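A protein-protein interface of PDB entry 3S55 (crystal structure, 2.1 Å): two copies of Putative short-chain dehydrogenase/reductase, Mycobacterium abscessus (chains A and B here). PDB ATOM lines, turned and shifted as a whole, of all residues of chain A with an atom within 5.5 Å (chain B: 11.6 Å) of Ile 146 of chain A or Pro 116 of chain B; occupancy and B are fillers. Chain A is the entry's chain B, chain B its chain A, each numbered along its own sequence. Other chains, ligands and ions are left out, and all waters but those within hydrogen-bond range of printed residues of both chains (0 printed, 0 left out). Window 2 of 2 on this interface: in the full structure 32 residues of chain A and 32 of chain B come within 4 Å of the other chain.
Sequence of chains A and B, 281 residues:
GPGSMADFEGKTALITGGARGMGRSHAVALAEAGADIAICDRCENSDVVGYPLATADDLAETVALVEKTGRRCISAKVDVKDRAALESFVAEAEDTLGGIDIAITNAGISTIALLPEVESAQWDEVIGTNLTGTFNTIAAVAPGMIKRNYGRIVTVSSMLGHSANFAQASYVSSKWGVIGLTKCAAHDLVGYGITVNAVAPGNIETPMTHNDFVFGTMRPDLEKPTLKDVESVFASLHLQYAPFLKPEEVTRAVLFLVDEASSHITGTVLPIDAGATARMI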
ATOM      1  N   ARG A  83      16.290   2.965  21.967  1.00  0.00           N
ATOM      2  CA  ARG A  83      15.454   3.043  23.164  1.00  0.00           C
ATOM      3  C   ARG A  83      16.254   3.024  24.463  1.00  0.00           C
ATOM      4  O   ARG A  83      15.966   3.788  25.392  1.00  0.00           O
ATOM      5  CB  ARG A  83      14.450   1.896  23.203  1.00  0.00           C
ATOM      6  CG  ARG A  83      13.388   2.088  24.297  1.00  0.00           C
ATOM      7  CD  ARG A  83      12.446   0.945  24.267  1.00  0.00           C
ATOM      8  NE  ARG A  83      11.374   1.039  25.249  1.00  0.00           N
ATOM      9  CZ  ARG A  83      10.334   0.212  25.280  1.00  0.00           C
ATOM     10  NH1 ARG A  83      10.238  -0.765  24.382  1.00  0.00           N
ATOM     11  NH2 ARG A  83       9.379   0.366  26.196  1.00  0.00           N
ATOM     12  N   ILE A 138       8.544   8.446  24.415  1.00  0.00           N
ATOM     13  CA  ILE A 138       7.390   8.297  25.294  1.00  0.00           C
ATOM     14  C   ILE A 138       7.615   7.129  26.224  1.00  0.00           C
ATOM     15  O   ILE A 138       7.380   7.236  27.434  1.00  0.00           O
ATOM     16  CB  ILE A 138       6.077   8.066  24.522  1.00  0.00           C
ATOM     17  CG1 ILE A 138       5.606   9.340  23.863  1.00  0.00           C
ATOM     18  CG2 ILE A 138       4.987   7.653  25.482  1.00  0.00           C
ATOM     19  CD1 ILE A 138       4.591   9.134  22.777  1.00  0.00           C
ATOM     20  N   ALA A 139       8.073   6.016  25.655  1.00  0.00           N
ATOM     21  CA  ALA A 139       8.321   4.812  26.454  1.00  0.00           C
ATOM     22  C   ALA A 139       9.426   5.075  27.480  1.00  0.00           C
ATOM     23  O   ALA A 139       9.394   4.535  28.565  1.00  0.00           O
ATOM     24  CB  ALA A 139       8.674   3.624  25.553  1.00  0.00           C
ATOM     25  N   VAL A 141      10.054   8.049  29.027  1.00  0.00           N
ATOM     26  CA  VAL A 141       9.638   8.990  30.079  1.00  0.00           C
ATOM     27  C   VAL A 141       8.460   8.560  30.904  1.00  0.00           C
ATOM     28  O   VAL A 141       8.357   8.953  32.078  1.00  0.00           O
ATOM     29  CB  VAL A 141       9.340  10.457  29.561  1.00  0.00           C
ATOM     30  CG1 VAL A 141      10.618  11.137  29.201  1.00  0.00           C
ATOM     31  CG2 VAL A 141       8.342  10.456  28.411  1.00  0.00           C
ATOM     32  N   ALA A 142       7.588   7.757  30.313  1.00  0.00           N
ATOM     33  CA  ALA A 142       6.305   7.373  30.952  1.00  0.00           C
ATOM     34  C   ALA A 142       6.397   6.646  32.287  1.00  0.00           C
ATOM     35  O   ALA A 142       5.583   6.929  33.156  1.00  0.00           O
ATOM     36  CB  ALA A 142       5.378   6.613  29.979  1.00  0.00           C
ATOM     37  N   PRO A 143       7.378   5.735  32.467  1.00  0.00           N
ATOM     38  CA  PRO A 143       7.450   5.051  33.754  1.00  0.00           C
ATOM     39  C   PRO A 143       7.549   6.018  34.922  1.00  0.00           C
ATOM     40  O   PRO A 143       6.841   5.818  35.900  1.00  0.00           O
ATOM     41  CB  PRO A 143       8.738   4.211  33.646  1.00  0.00           C
ATOM     42  CG  PRO A 143       8.902   3.980  32.133  1.00  0.00           C
ATOM     43  CD  PRO A 143       8.440   5.275  31.543  1.00  0.00           C
ATOM     44  N   GLY A 144       8.431   7.028  34.826  1.00  0.00           N
ATOM     45  CA  GLY A 144       8.599   8.030  35.878  1.00  0.00           C
ATOM     46  C   GLY A 144       7.380   8.949  35.995  1.00  0.00           C
ATOM     47  O   GLY A 144       7.011   9.348  37.115  1.00  0.00           O
ATOM     48  N   MET A 145       6.753   9.306  34.859  1.00  0.00           N
ATOM     49  CA  MET A 145       5.534  10.135  34.938  1.00  0.00           C
ATOM     50  C   MET A 145       4.411   9.385  35.616  1.00  0.00           C
ATOM     51  O   MET A 145       3.679   9.951  36.426  1.00  0.00           O
ATOM     52  CB  MET A 145       5.108  10.674  33.572  1.00  0.00           C
ATOM     53  CG  MET A 145       6.146  11.627  32.965  1.00  0.00           C
ATOM     54  SD  MET A 145       5.846  12.098  31.243  1.00  0.00           S
ATOM     55  CE  MET A 145       6.959  13.501  31.071  1.00  0.00           C
ATOM     56  N   ILE A 146       4.264   8.103  35.278  1.00  0.00           N
ATOM     57  CA  ILE A 146       3.277   7.235  35.922  1.00  0.00           C
ATOM     58  C   ILE A 146       3.553   7.148  37.432  1.00  0.00           C
ATOM     59  O   ILE A 146       2.670   7.401  38.226  1.00  0.00           O
ATOM     60  CB  ILE A 146       3.264   5.828  35.313  1.00  0.00           C
ATOM     61  CG1 ILE A 146       2.799   5.871  33.856  1.00  0.00           C
ATOM     62  CG2 ILE A 146       2.337   4.868  36.135  1.00  0.00           C
ATOM     63  CD1 ILE A 146       2.971   4.475  33.122  1.00  0.00           C
ATOM     64  N   LYS A 147       4.799   6.837  37.796  1.00  0.00           N
ATOM     65  CA  LYS A 147       5.246   6.772  39.180  1.00  0.00           C
ATOM     66  C   LYS A 147       4.942   8.078  39.933  1.00  0.00           C
ATOM     67  O   LYS A 147       4.456   8.057  41.075  1.00  0.00           O
ATOM     68  CB  LYS A 147       6.759   6.479  39.219  1.00  0.00           C
ATOM     69  N   ARG A 148       5.218   9.213  39.283  1.00  0.00           N
ATOM     70  CA  ARG A 148       5.003  10.536  39.912  1.00  0.00           C
ATOM     71  C   ARG A 148       3.583  11.069  39.730  1.00  0.00           C
ATOM     72  O   ARG A 148       3.233  12.097  40.322  1.00  0.00           O
ATOM     73  CB  ARG A 148       6.006  11.558  39.381  1.00  0.00           C
ATOM     74  CG  ARG A 148       7.453  11.299  39.817  1.00  0.00           C
ATOM     75  CD  ARG A 148       8.441  12.341  39.230  1.00  0.00           C
ATOM     76  NE  ARG A 148       8.578  12.264  37.793  1.00  0.00           N
ATOM     77  CZ  ARG A 148       9.379  11.414  37.134  1.00  0.00           C
ATOM     78  NH1 ARG A 148      10.129  10.540  37.790  1.00  0.00           N
ATOM     79  NH2 ARG A 148       9.441  11.445  35.805  1.00  0.00           N
ATOM     80  N   ASN A 149       2.796  10.388  38.883  1.00  0.00           N
ATOM     81  CA  ASN A 149       1.446  10.805  38.545  1.00  0.00           C
ATOM     82  C   ASN A 149       1.323  12.212  37.963  1.00  0.00           C
ATOM     83  O   ASN A 149       0.415  12.960  38.346  1.00  0.00           O
ATOM     84  CB  ASN A 149       0.512  10.674  39.743  1.00  0.00           C
ATOM     85  CG  ASN A 149      -0.912  10.358  39.316  1.00  0.00           C
ATOM     86  OD1 ASN A 149      -1.740  11.276  39.035  1.00  0.00           O
ATOM     87  ND2 ASN A 149      -1.206   9.067  39.211  1.00  0.00           N
ATOM     88  N   TYR A 150       2.206  12.554  37.018  1.00  0.00           N
ATOM     89  CA  TYR A 150       2.223  13.889  36.375  1.00  0.00           C
ATOM     90  C   TYR A 150       3.109  13.862  35.132  1.00  0.00           C
ATOM     91  O   TYR A 150       4.291  13.482  35.188  1.00  0.00           O
ATOM     92  CB  TYR A 150       2.676  15.040  37.322  1.00  0.00           C
ATOM     93  CG  TYR A 150       2.493  16.400  36.657  1.00  0.00           C
ATOM     94  CD1 TYR A 150       1.266  17.087  36.731  1.00  0.00           C
ATOM     95  CD2 TYR A 150       3.510  16.965  35.887  1.00  0.00           C
ATOM     96  CE1 TYR A 150       1.094  18.330  36.063  1.00  0.00           C
ATOM     97  CE2 TYR A 150       3.343  18.162  35.230  1.00  0.00           C
ATOM     98  CZ  TYR A 150       2.141  18.852  35.306  1.00  0.00           C
ATOM     99  OH  TYR A 150       2.001  20.082  34.640  1.00  0.00           O
ATOM    100  N   LEU A 189      -1.945   6.427  29.135  1.00  0.00           N
ATOM    101  CA  LEU A 189      -1.339   7.224  30.198  1.00  0.00           C
ATOM    102  C   LEU A 189      -2.378   8.009  31.011  1.00  0.00           C
ATOM    103  O   LEU A 189      -2.056   8.591  32.036  1.00  0.00           O
ATOM    104  CB  LEU A 189      -0.267   8.143  29.591  1.00  0.00           C
ATOM    105  CG  LEU A 189       0.944   7.417  28.911  1.00  0.00           C
ATOM    106  CD1 LEU A 189       2.038   8.395  28.492  1.00  0.00           C
ATOM    107  CD2 LEU A 189       1.536   6.326  29.804  1.00  0.00           C
ATOM    108  N   TYR A 192      -3.014   8.537  34.968  1.00  0.00           N
ATOM    109  CA  TYR A 192      -1.854   8.945  35.774  1.00  0.00           C
ATOM    110  C   TYR A 192      -1.501  10.421  35.700  1.00  0.00           C
ATOM    111  O   TYR A 192      -0.345  10.789  35.935  1.00  0.00           O
ATOM    112  CB  TYR A 192      -0.614   8.124  35.393  1.00  0.00           C
ATOM    113  CG  TYR A 192      -0.851   6.635  35.361  1.00  0.00           C
ATOM    114  CD1 TYR A 192      -1.116   5.931  36.529  1.00  0.00           C
ATOM    115  CD2 TYR A 192      -0.799   5.938  34.167  1.00  0.00           C
ATOM    116  CE1 TYR A 192      -1.319   4.582  36.508  1.00  0.00           C
ATOM    117  CE2 TYR A 192      -0.999   4.580  34.137  1.00  0.00           C
ATOM    118  CZ  TYR A 192      -1.262   3.904  35.307  1.00  0.00           C
ATOM    119  OH  TYR A 192      -1.475   2.536  35.276  1.00  0.00           O
ATOM    120  N   ILE A 194      -1.244  12.359  33.182  1.00  0.00           N
ATOM    121  CA  ILE A 194      -0.370  12.576  32.030  1.00  0.00           C
ATOM    122  C   ILE A 194      -1.231  12.897  30.826  1.00  0.00           C
ATOM    123  O   ILE A 194      -2.191  12.152  30.546  1.00  0.00           O
ATOM    124  CB  ILE A 194       0.442  11.312  31.711  1.00  0.00           C
ATOM    125  CG1 ILE A 194       1.318  10.921  32.923  1.00  0.00           C
ATOM    126  CG2 ILE A 194       1.305  11.542  30.479  1.00  0.00           C
ATOM    127  CD1 ILE A 194       1.821   9.463  32.900  1.00  0.00           C
ATOM    128  N   ILE B 112      -1.697  -6.538  21.479  1.00  0.00           N
ATOM    129  CA  ILE B 112      -2.283  -5.856  22.619  1.00  0.00           C
ATOM    130  C   ILE B 112      -1.209  -5.744  23.676  1.00  0.00           C
ATOM    131  O   ILE B 112      -0.708  -6.762  24.185  1.00  0.00           O
ATOM    132  CB  ILE B 112      -3.444  -6.645  23.231  1.00  0.00           C
ATOM    133  CG1 ILE B 112      -4.570  -6.838  22.203  1.00  0.00           C
ATOM    134  CG2 ILE B 112      -3.978  -5.909  24.509  1.00  0.00           C
ATOM    135  CD1 ILE B 112      -5.168  -8.237  22.212  1.00  0.00           C
ATOM    136  N   ALA B 113      -0.841  -4.503  23.988  1.00  0.00           N
ATOM    137  CA  ALA B 113       0.144  -4.207  25.025  1.00  0.00           C
ATOM    138  C   ALA B 113       0.077  -2.723  25.333  1.00  0.00           C
ATOM    139  O   ALA B 113       0.098  -1.891  24.414  1.00  0.00           O
ATOM    140  CB  ALA B 113       1.535  -4.564  24.555  1.00  0.00           C
ATOM    141  N   LEU B 114       0.007  -2.413  26.622  1.00  0.00           N
ATOM    142  CA  LEU B 114      -0.052  -1.029  27.129  1.00  0.00           C
ATOM    143  C   LEU B 114       1.317  -0.352  27.139  1.00  0.00           C
ATOM    144  O   LEU B 114       2.302  -0.974  27.501  1.00  0.00           O
ATOM    145  CB  LEU B 114      -0.618  -1.017  28.557  1.00  0.00           C
ATOM    146  CG  LEU B 114      -2.134  -1.175  28.729  1.00  0.00           C
ATOM    147  CD1 LEU B 114      -2.524  -1.823  30.080  1.00  0.00           C
ATOM    148  CD2 LEU B 114      -2.848   0.172  28.579  1.00  0.00           C
ATOM    149  N   LEU B 115       1.366   0.924  26.766  1.00  0.00           N
ATOM    150  CA  LEU B 115       2.571   1.772  27.004  1.00  0.00           C
ATOM    151  C   LEU B 115       2.746   1.957  28.527  1.00  0.00           C
ATOM    152  O   LEU B 115       1.746   1.925  29.235  1.00  0.00           O
ATOM    153  CB  LEU B 115       2.389   3.138  26.333  1.00  0.00           C
ATOM    154  CG  LEU B 115       2.587   3.318  24.820  1.00  0.00           C
ATOM    155  CD1 LEU B 115       1.992   4.654  24.358  1.00  0.00           C
ATOM    156  CD2 LEU B 115       4.072   3.267  24.464  1.00  0.00           C
ATOM    157  N   PRO B 116       3.995   2.109  29.053  1.00  0.00           N
ATOM    158  CA  PRO B 116       5.357   2.079  28.471  1.00  0.00           C
ATOM    159  C   PRO B 116       5.910   0.666  28.254  1.00  0.00           C
ATOM    160  O   PRO B 116       7.006   0.549  27.697  1.00  0.00           O
ATOM    161  CB  PRO B 116       6.213   2.743  29.557  1.00  0.00           C
ATOM    162  CG  PRO B 116       5.554   2.276  30.832  1.00  0.00           C
ATOM    163  CD  PRO B 116       4.059   2.360  30.514  1.00  0.00           C
ATOM    164  N   GLU B 117       5.179  -0.375  28.685  1.00  0.00           N
ATOM    165  CA  GLU B 117       5.673  -1.767  28.592  1.00  0.00           C
ATOM    166  C   GLU B 117       5.310  -2.461  27.273  1.00  0.00           C
ATOM    167  O   GLU B 117       4.808  -3.597  27.256  1.00  0.00           O
ATOM    168  CB  GLU B 117       5.206  -2.607  29.791  1.00  0.00           C
ATOM    169  N   VAL B 118       5.549  -1.766  26.168  1.00  0.00           N
ATOM    170  CA  VAL B 118       5.441  -2.361  24.838  1.00  0.00           C
ATOM    171  C   VAL B 118       6.862  -2.768  24.491  1.00  0.00           C
ATOM    172  O   VAL B 118       7.769  -1.959  24.624  1.00  0.00           O
ATOM    173  CB  VAL B 118       4.874  -1.359  23.804  1.00  0.00           C
ATOM    174  CG1 VAL B 118       4.904  -1.951  22.382  1.00  0.00           C
ATOM    175  CG2 VAL B 118       3.453  -0.980  24.191  1.00  0.00           C
ATOM    176  N   GLU B 119       7.067  -4.021  24.099  1.00  0.00           N
ATOM    177  CA  GLU B 119       8.432  -4.500  23.825  1.00  0.00           C
ATOM    178  C   GLU B 119       8.884  -3.941  22.477  1.00  0.00           C
ATOM    179  O   GLU B 119       8.105  -3.933  21.559  1.00  0.00           O
ATOM    180  CB  GLU B 119       8.499  -6.049  23.811  1.00  0.00           C
ATOM    181  CG  GLU B 119       8.294  -6.733  25.164  1.00  0.00           C
ATOM    182  CD  GLU B 119       9.405  -6.435  26.175  1.00  0.00           C
ATOM    183  OE1 GLU B 119      10.544  -6.072  25.773  1.00  0.00           O
ATOM    184  OE2 GLU B 119       9.145  -6.573  27.395  1.00  0.00           O
ATOM    185  N   SER B 120      10.126  -3.466  22.377  1.00  0.00           N
ATOM    186  CA  SER B 120      10.659  -2.945  21.093  1.00  0.00           C
ATOM    187  C   SER B 120      10.469  -3.948  19.947  1.00  0.00           C
ATOM    188  O   SER B 120      10.075  -3.567  18.848  1.00  0.00           O
ATOM    189  CB  SER B 120      12.140  -2.559  21.214  1.00  0.00           C
ATOM    190  OG  SER B 120      12.258  -1.328  21.914  1.00  0.00           O
ATOM    191  N   ALA B 121      10.700  -5.237  20.224  1.00  0.00           N
ATOM    192  CA  ALA B 121      10.555  -6.271  19.182  1.00  0.00           C
ATOM    193  C   ALA B 121       9.124  -6.358  18.654  1.00  0.00           C
ATOM    194  O   ALA B 121       8.905  -6.654  17.470  1.00  0.00           O
ATOM    195  CB  ALA B 121      11.037  -7.646  19.677  1.00  0.00           C
ATOM    196  N   GLN B 122       8.155  -6.105  19.536  1.00  0.00           N
ATOM    197  CA  GLN B 122       6.741  -6.156  19.156  1.00  0.00           C
ATOM    198  C   GLN B 122       6.367  -4.923  18.323  1.00  0.00           C
ATOM    199  O   GLN B 122       5.732  -5.042  17.269  1.00  0.00           O
ATOM    200  CB  GLN B 122       5.844  -6.257  20.381  1.00  0.00           C
ATOM    201  CG  GLN B 122       4.363  -6.522  20.041  1.00  0.00           C
ATOM    202  CD  GLN B 122       3.516  -6.726  21.283  1.00  0.00           C
ATOM    203  OE1 GLN B 122       3.239  -5.785  22.003  1.00  0.00           O
ATOM    204  NE2 GLN B 122       3.127  -7.967  21.544  1.00  0.00           N
ATOM    205  N   TRP B 123       6.770  -3.748  18.810  1.00  0.00           N
ATOM    206  CA  TRP B 123       6.660  -2.527  18.036  1.00  0.00           C
ATOM    207  C   TRP B 123       7.235  -2.736  16.639  1.00  0.00           C
ATOM    208  O   TRP B 123       6.606  -2.384  15.654  1.00  0.00           O
ATOM    209  CB  TRP B 123       7.393  -1.373  18.745  1.00  0.00           C
ATOM    210  CG  TRP B 123       7.442  -0.113  17.928  1.00  0.00           C
ATOM    211  CD1 TRP B 123       8.437   0.277  17.093  1.00  0.00           C
ATOM    212  CD2 TRP B 123       6.428   0.920  17.854  1.00  0.00           C
ATOM    213  NE1 TRP B 123       8.141   1.501  16.527  1.00  0.00           N
ATOM    214  CE2 TRP B 123       6.905   1.908  16.958  1.00  0.00           C
ATOM    215  CE3 TRP B 123       5.177   1.107  18.467  1.00  0.00           C
ATOM    216  CZ2 TRP B 123       6.163   3.064  16.639  1.00  0.00           C
ATOM    217  CZ3 TRP B 123       4.439   2.257  18.152  1.00  0.00           C
ATOM    218  CH2 TRP B 123       4.937   3.216  17.248  1.00  0.00           C
ATOM    219  N   PHE B 166      -7.118   1.822  24.047  1.00  0.00           N
ATOM    220  CA  PHE B 166      -6.097   1.447  24.993  1.00  0.00           C
ATOM    221  C   PHE B 166      -5.229   0.290  24.480  1.00  0.00           C
ATOM    222  O   PHE B 166      -5.705  -0.585  23.766  1.00  0.00           O
ATOM    223  CB  PHE B 166      -6.722   1.004  26.309  1.00  0.00           C
ATOM    224  CG  PHE B 166      -7.572   2.048  26.955  1.00  0.00           C
ATOM    225  CD1 PHE B 166      -6.990   3.040  27.754  1.00  0.00           C
ATOM    226  CD2 PHE B 166      -8.959   2.040  26.770  1.00  0.00           C
ATOM    227  CE1 PHE B 166      -7.786   4.021  28.368  1.00  0.00           C
ATOM    228  CE2 PHE B 166      -9.767   3.000  27.375  1.00  0.00           C
ATOM    229  CZ  PHE B 166      -9.172   3.997  28.172  1.00  0.00           C
ATOM    230  N   ALA B 167      -3.960   0.302  24.886  1.00  0.00           N
ATOM    231  CA  ALA B 167      -3.056  -0.832  24.722  1.00  0.00           C
ATOM    232  C   ALA B 167      -2.862  -1.197  23.249  1.00  0.00           C
ATOM    233  O   ALA B 167      -2.669  -2.356  22.914  1.00  0.00           O
ATOM    234  CB  ALA B 167      -3.564  -2.043  25.505  1.00  0.00           C
ATOM    235  N   GLN B 168      -2.916  -0.194  22.378  1.00  0.00           N
ATOM    236  CA  GLN B 168      -2.886  -0.450  20.940  1.00  0.00           C
ATOM    237  C   GLN B 168      -1.858   0.368  20.195  1.00  0.00           C
ATOM    238  O   GLN B 168      -1.909   0.432  18.969  1.00  0.00           O
ATOM    239  CB  GLN B 168      -4.282  -0.236  20.324  1.00  0.00           C
ATOM    240  CG  GLN B 168      -5.243  -1.353  20.636  1.00  0.00           C
ATOM    241  CD  GLN B 168      -4.775  -2.650  20.080  1.00  0.00           C
ATOM    242  OE1 GLN B 168      -3.738  -2.717  19.434  1.00  0.00           O
ATOM    243  NE2 GLN B 168      -5.536  -3.692  20.302  1.00  0.00           N
ATOM    244  N   ALA B 169      -0.910   0.963  20.919  1.00  0.00           N
ATOM    245  CA  ALA B 169       0.037   1.913  20.306  1.00  0.00           C
ATOM    246  C   ALA B 169       0.672   1.408  18.992  1.00  0.00           C
ATOM    247  O   ALA B 169       0.745   2.151  18.007  1.00  0.00           O
ATOM    248  CB  ALA B 169       1.131   2.345  21.323  1.00  0.00           C
ATOM    249  N   SER B 170       1.131   0.161  18.977  1.00  0.00           N
ATOM    250  CA  SER B 170       1.843  -0.381  17.800  1.00  0.00           C
ATOM    251  C   SER B 170       0.886  -0.522  16.630  1.00  0.00           C
ATOM    252  O   SER B 170       1.147  -0.031  15.535  1.00  0.00           O
ATOM    253  CB  SER B 170       2.444  -1.762  18.087  1.00  0.00           C
ATOM    254  OG  SER B 170       3.507  -1.681  19.014  1.00  0.00           O
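Of the printed residues of chain B, Arg 83 of chain A touches Pro 116, Val 118, Glu 119 and Ser 120. Of the printed residues of chain B, Ala 139 of chain A touches Pro 116. Pro 143 of chain A touches one residue of chain B. No residue of chain B comes within 4 Å of Gly 144 of chain A. Met 145 of chain A touches none of the printed residues of chain B. No residue of chain B comes within 4 Å of Lys 147 of chain A. No residue of chain B comes within 4 Å of Arg 148 of chain A. No residue of chain B comes within 4 Å of Asn 149 of chain A. No residue of chain B comes within 4 Å of Leu 189 of chain A. No residue of chain B comes within 4 Å of Tyr 192 of chain A. Ile 194 of chain A touches none of the printed residues of chain B. Leu 114 of chain B touches none of the printed residues of chain A. Of the printed residues of chain A, Val 118 of chain B touches Arg 83 (2.8 Å). The nearest residue of chain B that does not touch Ile 146 of chain A is Leu 115 of chain B (4.8 Å). The nearest printed residue of chain A that does not touch Pro 116 of chain B is Leu 189 of chain A (4.8 Å). The nearest printed residue of chain B that does not touch Ala 142 of chain A is Leu 115 of chain B (5.5 Å).
No position is printed for both chains. Of the 8 pairs that touch across the chains among the printed residues, none has its exchanged pair printed and touching as well.
The backbone carbonyl oxygen (O) of Pro 116 of chain B is in hydrogen-bond range of the guanidinium group (NH2) of Arg 83 of chain A (2.8 Å). The backbone carbonyl oxygen (O) of Val 118 of chain B lies within hydrogen-bond range of the guanidinium group (NH1) of Arg 83 of chain A, 2.8 Å away. The guanidinium group (NH1) of Arg 83 of chain A lies within hydrogen-bond range of the side-chain hydroxyl (OG) of Ser 120 of chain B (3.2 Å).
Among the printed residues, merely in contact across the chains: Arg 83 of chain A with Glu 119 of chain B (3.9 Å), Ala 139 of chain A with Pro 116 of chain B (3.8 Å), Ala 142 of chain A with Pro 116 of chain B (3.98 Å), Pro 143 of chain A with Pro 116 of chain B (3.9 Å) and Ile 146 of chain A with Pro 116 of chain B (3.5 Å).
Of the 17 printed residues of chain B, 4 touch a printed residue of chain A. Hydrophobic or aromatic side chains of chain B that line the printed part of chain A: Pro 116. Along chain B the printed residues that touch a printed residue of chain A span positions 116 to 120. Of the 16 printed residues of chain A, 5 touch a printed residue of chain B. Hydrophobic or aromatic side chains of chain A within 4 Å of the printed part of chain B: Ala 142, Pro 143 and Ile 146. Among the printed residues, 8 pairs touch across the chains. Among the printed residues, no Asp or Glu carboxylate lies within 4 Å of a Lys or Arg side-chain nitrogen of the other chain.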
